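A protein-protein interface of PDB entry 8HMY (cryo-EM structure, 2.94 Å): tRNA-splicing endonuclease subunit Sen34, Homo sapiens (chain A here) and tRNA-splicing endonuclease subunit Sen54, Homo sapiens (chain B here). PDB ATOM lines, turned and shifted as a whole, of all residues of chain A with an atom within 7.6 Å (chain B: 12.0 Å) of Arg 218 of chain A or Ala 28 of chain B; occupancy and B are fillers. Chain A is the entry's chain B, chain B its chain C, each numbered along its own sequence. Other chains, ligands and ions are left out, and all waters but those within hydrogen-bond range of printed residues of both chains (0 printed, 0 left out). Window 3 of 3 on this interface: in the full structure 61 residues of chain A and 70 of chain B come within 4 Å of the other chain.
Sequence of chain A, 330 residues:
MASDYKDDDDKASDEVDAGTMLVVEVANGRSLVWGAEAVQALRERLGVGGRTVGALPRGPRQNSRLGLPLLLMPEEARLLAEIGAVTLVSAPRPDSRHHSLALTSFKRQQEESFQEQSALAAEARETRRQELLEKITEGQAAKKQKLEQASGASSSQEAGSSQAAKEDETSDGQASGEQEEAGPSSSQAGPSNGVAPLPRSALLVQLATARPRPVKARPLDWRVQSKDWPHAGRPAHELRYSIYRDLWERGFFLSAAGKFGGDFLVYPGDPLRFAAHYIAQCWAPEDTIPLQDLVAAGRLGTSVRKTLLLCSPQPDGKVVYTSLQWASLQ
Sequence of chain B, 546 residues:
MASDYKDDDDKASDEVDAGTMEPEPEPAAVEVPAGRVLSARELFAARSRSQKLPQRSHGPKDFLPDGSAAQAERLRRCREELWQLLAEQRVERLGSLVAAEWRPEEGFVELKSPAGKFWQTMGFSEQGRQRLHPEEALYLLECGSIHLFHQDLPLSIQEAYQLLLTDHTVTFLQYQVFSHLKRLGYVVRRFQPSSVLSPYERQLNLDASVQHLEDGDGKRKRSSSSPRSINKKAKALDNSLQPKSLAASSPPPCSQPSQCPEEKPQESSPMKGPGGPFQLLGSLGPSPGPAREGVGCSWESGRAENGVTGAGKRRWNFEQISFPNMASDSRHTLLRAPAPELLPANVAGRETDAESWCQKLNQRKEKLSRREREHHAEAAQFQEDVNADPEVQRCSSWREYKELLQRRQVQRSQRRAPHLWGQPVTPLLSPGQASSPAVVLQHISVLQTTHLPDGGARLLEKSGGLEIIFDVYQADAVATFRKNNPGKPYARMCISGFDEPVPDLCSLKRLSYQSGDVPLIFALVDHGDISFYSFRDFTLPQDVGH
The side-chain amino group (NZ) of Lys 216 of chain A lies within salt-bridge range of the side-chain carboxylate (OE2) of Glu 31 of chain B. The backbone carbonyl oxygen (O) of Val 215 of chain A lies close to the side-chain carboxylate (OE1) of Glu 31 of chain B, 3.4 Å away. The backbone carbonyl oxygen of Pro 92 of chain A sits close to the side-chain amide nitrogen of Gln 162 of chain B (2.3 Å). N of Val 32 of chain B lies within hydrogen-bond range of O of Val 215 of chain A, at 3.2 Å. O of Ala 217 of chain A sits at hydrogen-bond distance from N of Val 30 of chain B (2.6 Å).
N of Ser 90 of chain A is in hydrogen-bond range of O of Arg 218 of chain A, 3.5 Å away.
Val 89 of chain A touches Val 30 of chain B. Ala 91 of chain A touches Gln 162 of chain B. Lys 216 of chain A touches Val 30 of chain B (CA to O, 3.3 Å). Ala 29 of chain B touches Ala 217 of chain A. Ala 217 of chain A touches Val 32 of chain B (CB to CG2, 3.7 Å). CG of Arg 218 of chain A touches O of Ala 28 of chain B, at 3.3 Å. O of Ala 28 of chain B touches CD of Pro 219 of chain A, at 3.4 Å. CD of Pro 219 of chain A touches CA of Ala 29 of chain B (3.9 Å). CG2 of Val 30 of chain B touches CB of Pro 219 of chain A, at 3.8 Å.
Of chain B, only Val 30 (3.97 Å) comes within 4 Å of Val 89 of chain A. No residue of chain B comes within 4 Å of Ser 90 of chain A. Printed residues of chain B within 4 Å of Val 215 of chain A: Glu 31 and Val 32. Of chain B, only Ala 29 (3.5 Å), Val 30 (2.6 Å) and Val 32 (3.7 Å) come within 4 Å of Ala 217 of chain A. Of chain B, only Ala 28 comes within 4 Å of Arg 218 of chain A. Pro 219 of chain A touches three residues of chain B. No residue of chain B comes within 4 Å of Leu 220 of chain A. Ala 28 of chain B touches two residues of chain A. Of the printed residues of chain A, Glu 31 of chain B touches Val 215 (3.4 Å) and Lys 216 (3.9 Å). Of the printed residues of chain A, Gln 162 of chain B touches Ala 91 (3.9 Å) and Pro 92 (2.3 Å). The nearest residue of chain A that does not touch Ala 28 of chain B is Ala 217 of chain A (5.2 Å).
Of the 14 printed residues of chain A, 8 touch a printed residue of chain B. Printed residues of chain A that touch a printed residue of chain B: Val 89, Ala 91, Pro 92, Val 215, Lys 216, Ala 217, Arg 218 and Pro 219. Hydrophobic or aromatic side chains of chain B within 4 Å of the printed part of chain A: Val 30 and Val 32. Along chain B the printed residues that touch a printed residue of chain A span positions 28 to 162. Among the printed residues, Asp or Glu carboxylates within 4 Å of a Lys or Arg side-chain nitrogen of the other chain: Lys 216 of chain A with Glu 31 of chain B (3.95 Å).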
ATOM      1  N   THR A  87     -31.048  25.129  -0.551  1.00  0.00           N
ATOM      2  CA  THR A  87     -30.010  25.400  -1.542  1.00  0.00           C
ATOM      3  C   THR A  87     -28.661  25.302  -0.839  1.00  0.00           C
ATOM      4  O   THR A  87     -28.256  26.231  -0.138  1.00  0.00           O
ATOM      5  CB  THR A  87     -30.195  26.772  -2.181  1.00  0.00           C
ATOM      6  OG1 THR A  87     -29.721  27.781  -1.285  1.00  0.00           O
ATOM      7  CG2 THR A  87     -31.658  27.029  -2.478  1.00  0.00           C
ATOM      8  N   LEU A  88     -27.972  24.178  -1.018  1.00  0.00           N
ATOM      9  CA  LEU A  88     -26.647  24.024  -0.435  1.00  0.00           C
ATOM     10  C   LEU A  88     -25.675  25.019  -1.052  1.00  0.00           C
ATOM     11  O   LEU A  88     -25.674  25.243  -2.265  1.00  0.00           O
ATOM     12  CB  LEU A  88     -26.129  22.603  -0.645  1.00  0.00           C
ATOM     13  CG  LEU A  88     -26.929  21.447  -0.060  1.00  0.00           C
ATOM     14  CD1 LEU A  88     -26.457  20.144  -0.662  1.00  0.00           C
ATOM     15  CD2 LEU A  88     -26.790  21.413   1.443  1.00  0.00           C
ATOM     16  N   VAL A  89     -24.849  25.626  -0.206  1.00  0.00           N
ATOM     17  CA  VAL A  89     -23.765  26.493  -0.625  1.00  0.00           C
ATOM     18  C   VAL A  89     -22.492  26.025   0.070  1.00  0.00           C
ATOM     19  O   VAL A  89     -22.485  25.025   0.784  1.00  0.00           O
ATOM     20  CB  VAL A  89     -24.045  27.978  -0.324  1.00  0.00           C
ATOM     21  CG1 VAL A  89     -25.320  28.428  -1.002  1.00  0.00           C
ATOM     22  CG2 VAL A  89     -24.137  28.203   1.165  1.00  0.00           C
ATOM     23  N   SER A  90     -21.406  26.758  -0.151  1.00  0.00           N
ATOM     24  CA  SER A  90     -20.126  26.464   0.476  1.00  0.00           C
ATOM     25  C   SER A  90     -19.713  27.665   1.309  1.00  0.00           C
ATOM     26  O   SER A  90     -19.938  28.809   0.902  1.00  0.00           O
ATOM     27  CB  SER A  90     -19.061  26.131  -0.566  1.00  0.00           C
ATOM     28  OG  SER A  90     -18.766  27.265  -1.357  1.00  0.00           O
ATOM     29  N   ALA A  91     -19.132  27.399   2.476  1.00  0.00           N
ATOM     30  CA  ALA A  91     -18.850  28.444   3.447  1.00  0.00           C
ATOM     31  C   ALA A  91     -18.051  29.575   2.804  1.00  0.00           C
ATOM     32  O   ALA A  91     -16.944  29.337   2.303  1.00  0.00           O
ATOM     33  CB  ALA A  91     -18.082  27.865   4.634  1.00  0.00           C
ATOM     34  N   PRO A  92     -18.568  30.799   2.796  1.00  0.00           N
ATOM     35  CA  PRO A  92     -17.840  31.908   2.174  1.00  0.00           C
ATOM     36  C   PRO A  92     -16.590  32.257   2.963  1.00  0.00           C
ATOM     37  O   PRO A  92     -16.398  31.857   4.110  1.00  0.00           O
ATOM     38  CB  PRO A  92     -18.843  33.066   2.200  1.00  0.00           C
ATOM     39  CG  PRO A  92     -20.165  32.444   2.495  1.00  0.00           C
ATOM     40  CD  PRO A  92     -19.885  31.218   3.297  1.00  0.00           C
ATOM     41  N   VAL A 215     -23.501  37.775   2.881  1.00  0.00           N
ATOM     42  CA  VAL A 215     -22.334  37.400   2.093  1.00  0.00           C
ATOM     43  C   VAL A 215     -22.782  36.513   0.944  1.00  0.00           C
ATOM     44  O   VAL A 215     -23.657  35.656   1.112  1.00  0.00           O
ATOM     45  CB  VAL A 215     -21.270  36.681   2.949  1.00  0.00           C
ATOM     46  CG1 VAL A 215     -20.618  37.657   3.908  1.00  0.00           C
ATOM     47  CG2 VAL A 215     -21.887  35.520   3.703  1.00  0.00           C
ATOM     48  N   LYS A 216     -22.191  36.725  -0.225  1.00  0.00           N
ATOM     49  CA  LYS A 216     -22.496  35.898  -1.381  1.00  0.00           C
ATOM     50  C   LYS A 216     -21.687  34.612  -1.325  1.00  0.00           C
ATOM     51  O   LYS A 216     -20.458  34.645  -1.224  1.00  0.00           O
ATOM     52  CB  LYS A 216     -22.202  36.654  -2.673  1.00  0.00           C
ATOM     53  CG  LYS A 216     -22.664  38.096  -2.659  1.00  0.00           C
ATOM     54  CD  LYS A 216     -22.683  38.675  -4.058  1.00  0.00           C
ATOM     55  CE  LYS A 216     -23.878  38.166  -4.835  1.00  0.00           C
ATOM     56  NZ  LYS A 216     -25.154  38.525  -4.164  1.00  0.00           N
ATOM     57  N   ALA A 217     -22.379  33.480  -1.383  1.00  0.00           N
ATOM     58  CA  ALA A 217     -21.746  32.173  -1.402  1.00  0.00           C
ATOM     59  C   ALA A 217     -22.010  31.502  -2.740  1.00  0.00           C
ATOM     60  O   ALA A 217     -23.062  31.698  -3.353  1.00  0.00           O
ATOM     61  CB  ALA A 217     -22.257  31.288  -0.264  1.00  0.00           C
ATOM     62  N   ARG A 218     -21.043  30.718  -3.191  1.00  0.00           N
ATOM     63  CA  ARG A 218     -21.324  30.102  -4.479  1.00  0.00           C
ATOM     64  C   ARG A 218     -22.033  28.764  -4.286  1.00  0.00           C
ATOM     65  O   ARG A 218     -21.661  27.987  -3.403  1.00  0.00           O
ATOM     66  CB  ARG A 218     -20.039  29.899  -5.270  1.00  0.00           C
ATOM     67  CG  ARG A 218     -19.830  30.946  -6.348  1.00  0.00           C
ATOM     68  CD  ARG A 218     -18.378  31.044  -6.768  1.00  0.00           C
ATOM     69  NE  ARG A 218     -18.199  32.017  -7.842  1.00  0.00           N
ATOM     70  CZ  ARG A 218     -17.037  32.576  -8.159  1.00  0.00           C
ATOM     71  NH1 ARG A 218     -15.941  32.265  -7.481  1.00  0.00           N
ATOM     72  NH2 ARG A 218     -16.971  33.452  -9.153  1.00  0.00           N
ATOM     73  N   PRO A 219     -23.048  28.486  -5.104  1.00  0.00           N
ATOM     74  CA  PRO A 219     -23.865  27.284  -4.887  1.00  0.00           C
ATOM     75  C   PRO A 219     -23.063  26.011  -5.113  1.00  0.00           C
ATOM     76  O   PRO A 219     -22.330  25.883  -6.096  1.00  0.00           O
ATOM     77  CB  PRO A 219     -24.992  27.433  -5.913  1.00  0.00           C
ATOM     78  CG  PRO A 219     -24.445  28.337  -6.951  1.00  0.00           C
ATOM     79  CD  PRO A 219     -23.512  29.272  -6.257  1.00  0.00           C
ATOM     80  N   LEU A 220     -23.214  25.067  -4.190  1.00  0.00           N
ATOM     81  CA  LEU A 220     -22.494  23.806  -4.249  1.00  0.00           C
ATOM     82  C   LEU A 220     -23.245  22.801  -5.109  1.00  0.00           C
ATOM     83  O   LEU A 220     -24.476  22.727  -5.070  1.00  0.00           O
ATOM     84  CB  LEU A 220     -22.300  23.246  -2.841  1.00  0.00           C
ATOM     85  CG  LEU A 220     -21.538  21.934  -2.709  1.00  0.00           C
ATOM     86  CD1 LEU A 220     -20.107  22.128  -3.149  1.00  0.00           C
ATOM     87  CD2 LEU A 220     -21.590  21.429  -1.286  1.00  0.00           C
ATOM     88  N   ASP A 221     -22.497  22.029  -5.889  1.00  0.00           N
ATOM     89  CA  ASP A 221     -23.059  20.967  -6.716  1.00  0.00           C
ATOM     90  C   ASP A 221     -22.840  19.644  -5.995  1.00  0.00           C
ATOM     91  O   ASP A 221     -21.717  19.131  -5.949  1.00  0.00           O
ATOM     92  CB  ASP A 221     -22.421  20.954  -8.101  1.00  0.00           C
ATOM     93  CG  ASP A 221     -23.016  19.893  -9.002  1.00  0.00           C
ATOM     94  OD1 ASP A 221     -24.251  19.894  -9.186  1.00  0.00           O
ATOM     95  OD2 ASP A 221     -22.250  19.061  -9.528  1.00  0.00           O
ATOM     96  N   ASP A 228     -15.361  20.081  -0.687  1.00  0.00           N
ATOM     97  CA  ASP A 228     -16.415  20.493   0.230  1.00  0.00           C
ATOM     98  C   ASP A 228     -17.664  19.630   0.122  1.00  0.00           C
ATOM     99  O   ASP A 228     -18.680  19.953   0.743  1.00  0.00           O
ATOM    100  CB  ASP A 228     -16.773  21.959  -0.008  1.00  0.00           C
ATOM    101  CG  ASP A 228     -16.947  22.278  -1.475  1.00  0.00           C
ATOM    102  OD1 ASP A 228     -17.051  21.331  -2.280  1.00  0.00           O
ATOM    103  OD2 ASP A 228     -16.972  23.475  -1.827  1.00  0.00           O
ATOM    104  N   ALA B  28     -23.629  30.528 -10.735  1.00  0.00           N
ATOM    105  CA  ALA B  28     -23.774  31.911 -10.296  1.00  0.00           C
ATOM    106  C   ALA B  28     -23.260  32.084  -8.870  1.00  0.00           C
ATOM    107  O   ALA B  28     -22.225  31.525  -8.504  1.00  0.00           O
ATOM    108  CB  ALA B  28     -25.225  32.349 -10.394  1.00  0.00           C
ATOM    109  N   ALA B  29     -23.988  32.861  -8.070  1.00  0.00           N
ATOM    110  CA  ALA B  29     -23.615  33.109  -6.681  1.00  0.00           C
ATOM    111  C   ALA B  29     -24.878  33.369  -5.879  1.00  0.00           C
ATOM    112  O   ALA B  29     -25.664  34.253  -6.232  1.00  0.00           O
ATOM    113  CB  ALA B  29     -22.652  34.288  -6.568  1.00  0.00           C
ATOM    114  N   VAL B  30     -25.065  32.610  -4.808  1.00  0.00           N
ATOM    115  CA  VAL B  30     -26.254  32.701  -3.969  1.00  0.00           C
ATOM    116  C   VAL B  30     -26.015  33.724  -2.867  1.00  0.00           C
ATOM    117  O   VAL B  30     -24.915  33.832  -2.319  1.00  0.00           O
ATOM    118  CB  VAL B  30     -26.612  31.313  -3.397  1.00  0.00           C
ATOM    119  CG1 VAL B  30     -27.756  31.409  -2.409  1.00  0.00           C
ATOM    120  CG2 VAL B  30     -26.963  30.361  -4.520  1.00  0.00           C
ATOM    121  N   GLU B  31     -27.055  34.483  -2.537  1.00  0.00           N
ATOM    122  CA  GLU B  31     -27.000  35.496  -1.492  1.00  0.00           C
ATOM    123  C   GLU B  31     -27.518  34.892  -0.193  1.00  0.00           C
ATOM    124  O   GLU B  31     -28.618  34.330  -0.164  1.00  0.00           O
ATOM    125  CB  GLU B  31     -27.822  36.721  -1.885  1.00  0.00           C
ATOM    126  CG  GLU B  31     -28.145  37.657  -0.740  1.00  0.00           C
ATOM    127  CD  GLU B  31     -26.934  38.419  -0.251  1.00  0.00           C
ATOM    128  OE1 GLU B  31     -26.179  37.872   0.576  1.00  0.00           O
ATOM    129  OE2 GLU B  31     -26.735  39.567  -0.696  1.00  0.00           O
ATOM    130  N   VAL B  32     -26.731  35.007   0.872  1.00  0.00           N
ATOM    131  CA  VAL B  32     -27.028  34.345   2.141  1.00  0.00           C
ATOM    132  C   VAL B  32     -27.353  35.367   3.223  1.00  0.00           C
ATOM    133  O   VAL B  32     -26.463  35.727   4.006  1.00  0.00           O
ATOM    134  CB  VAL B  32     -25.851  33.467   2.589  1.00  0.00           C
ATOM    135  CG1 VAL B  32     -26.285  32.524   3.688  1.00  0.00           C
ATOM    136  CG2 VAL B  32     -25.289  32.704   1.415  1.00  0.00           C
ATOM    137  N   PRO B  33     -28.589  35.849   3.324  1.00  0.00           N
ATOM    138  CA  PRO B  33     -28.926  36.756   4.423  1.00  0.00           C
ATOM    139  C   PRO B  33     -28.911  36.015   5.747  1.00  0.00           C
ATOM    140  O   PRO B  33     -29.266  34.837   5.829  1.00  0.00           O
ATOM    141  CB  PRO B  33     -30.336  37.232   4.067  1.00  0.00           C
ATOM    142  CG  PRO B  33     -30.918  36.081   3.334  1.00  0.00           C
ATOM    143  CD  PRO B  33     -29.780  35.474   2.543  1.00  0.00           C
ATOM    144  N   GLN B 162     -16.055  28.696  11.750  1.00  0.00           N
ATOM    145  CA  GLN B 162     -15.481  28.554  10.416  1.00  0.00           C
ATOM    146  C   GLN B 162     -13.971  28.770  10.424  1.00  0.00           C
ATOM    147  O   GLN B 162     -13.225  28.026   9.779  1.00  0.00           O
ATOM    148  CB  GLN B 162     -16.155  29.542   9.468  1.00  0.00           C
ATOM    149  CG  GLN B 162     -15.657  29.485   8.049  1.00  0.00           C
ATOM    150  CD  GLN B 162     -16.386  30.457   7.157  1.00  0.00           C
ATOM    151  OE1 GLN B 162     -17.458  30.950   7.505  1.00  0.00           O
ATOM    152  NE2 GLN B 162     -15.809  30.746   6.001  1.00  0.00           N
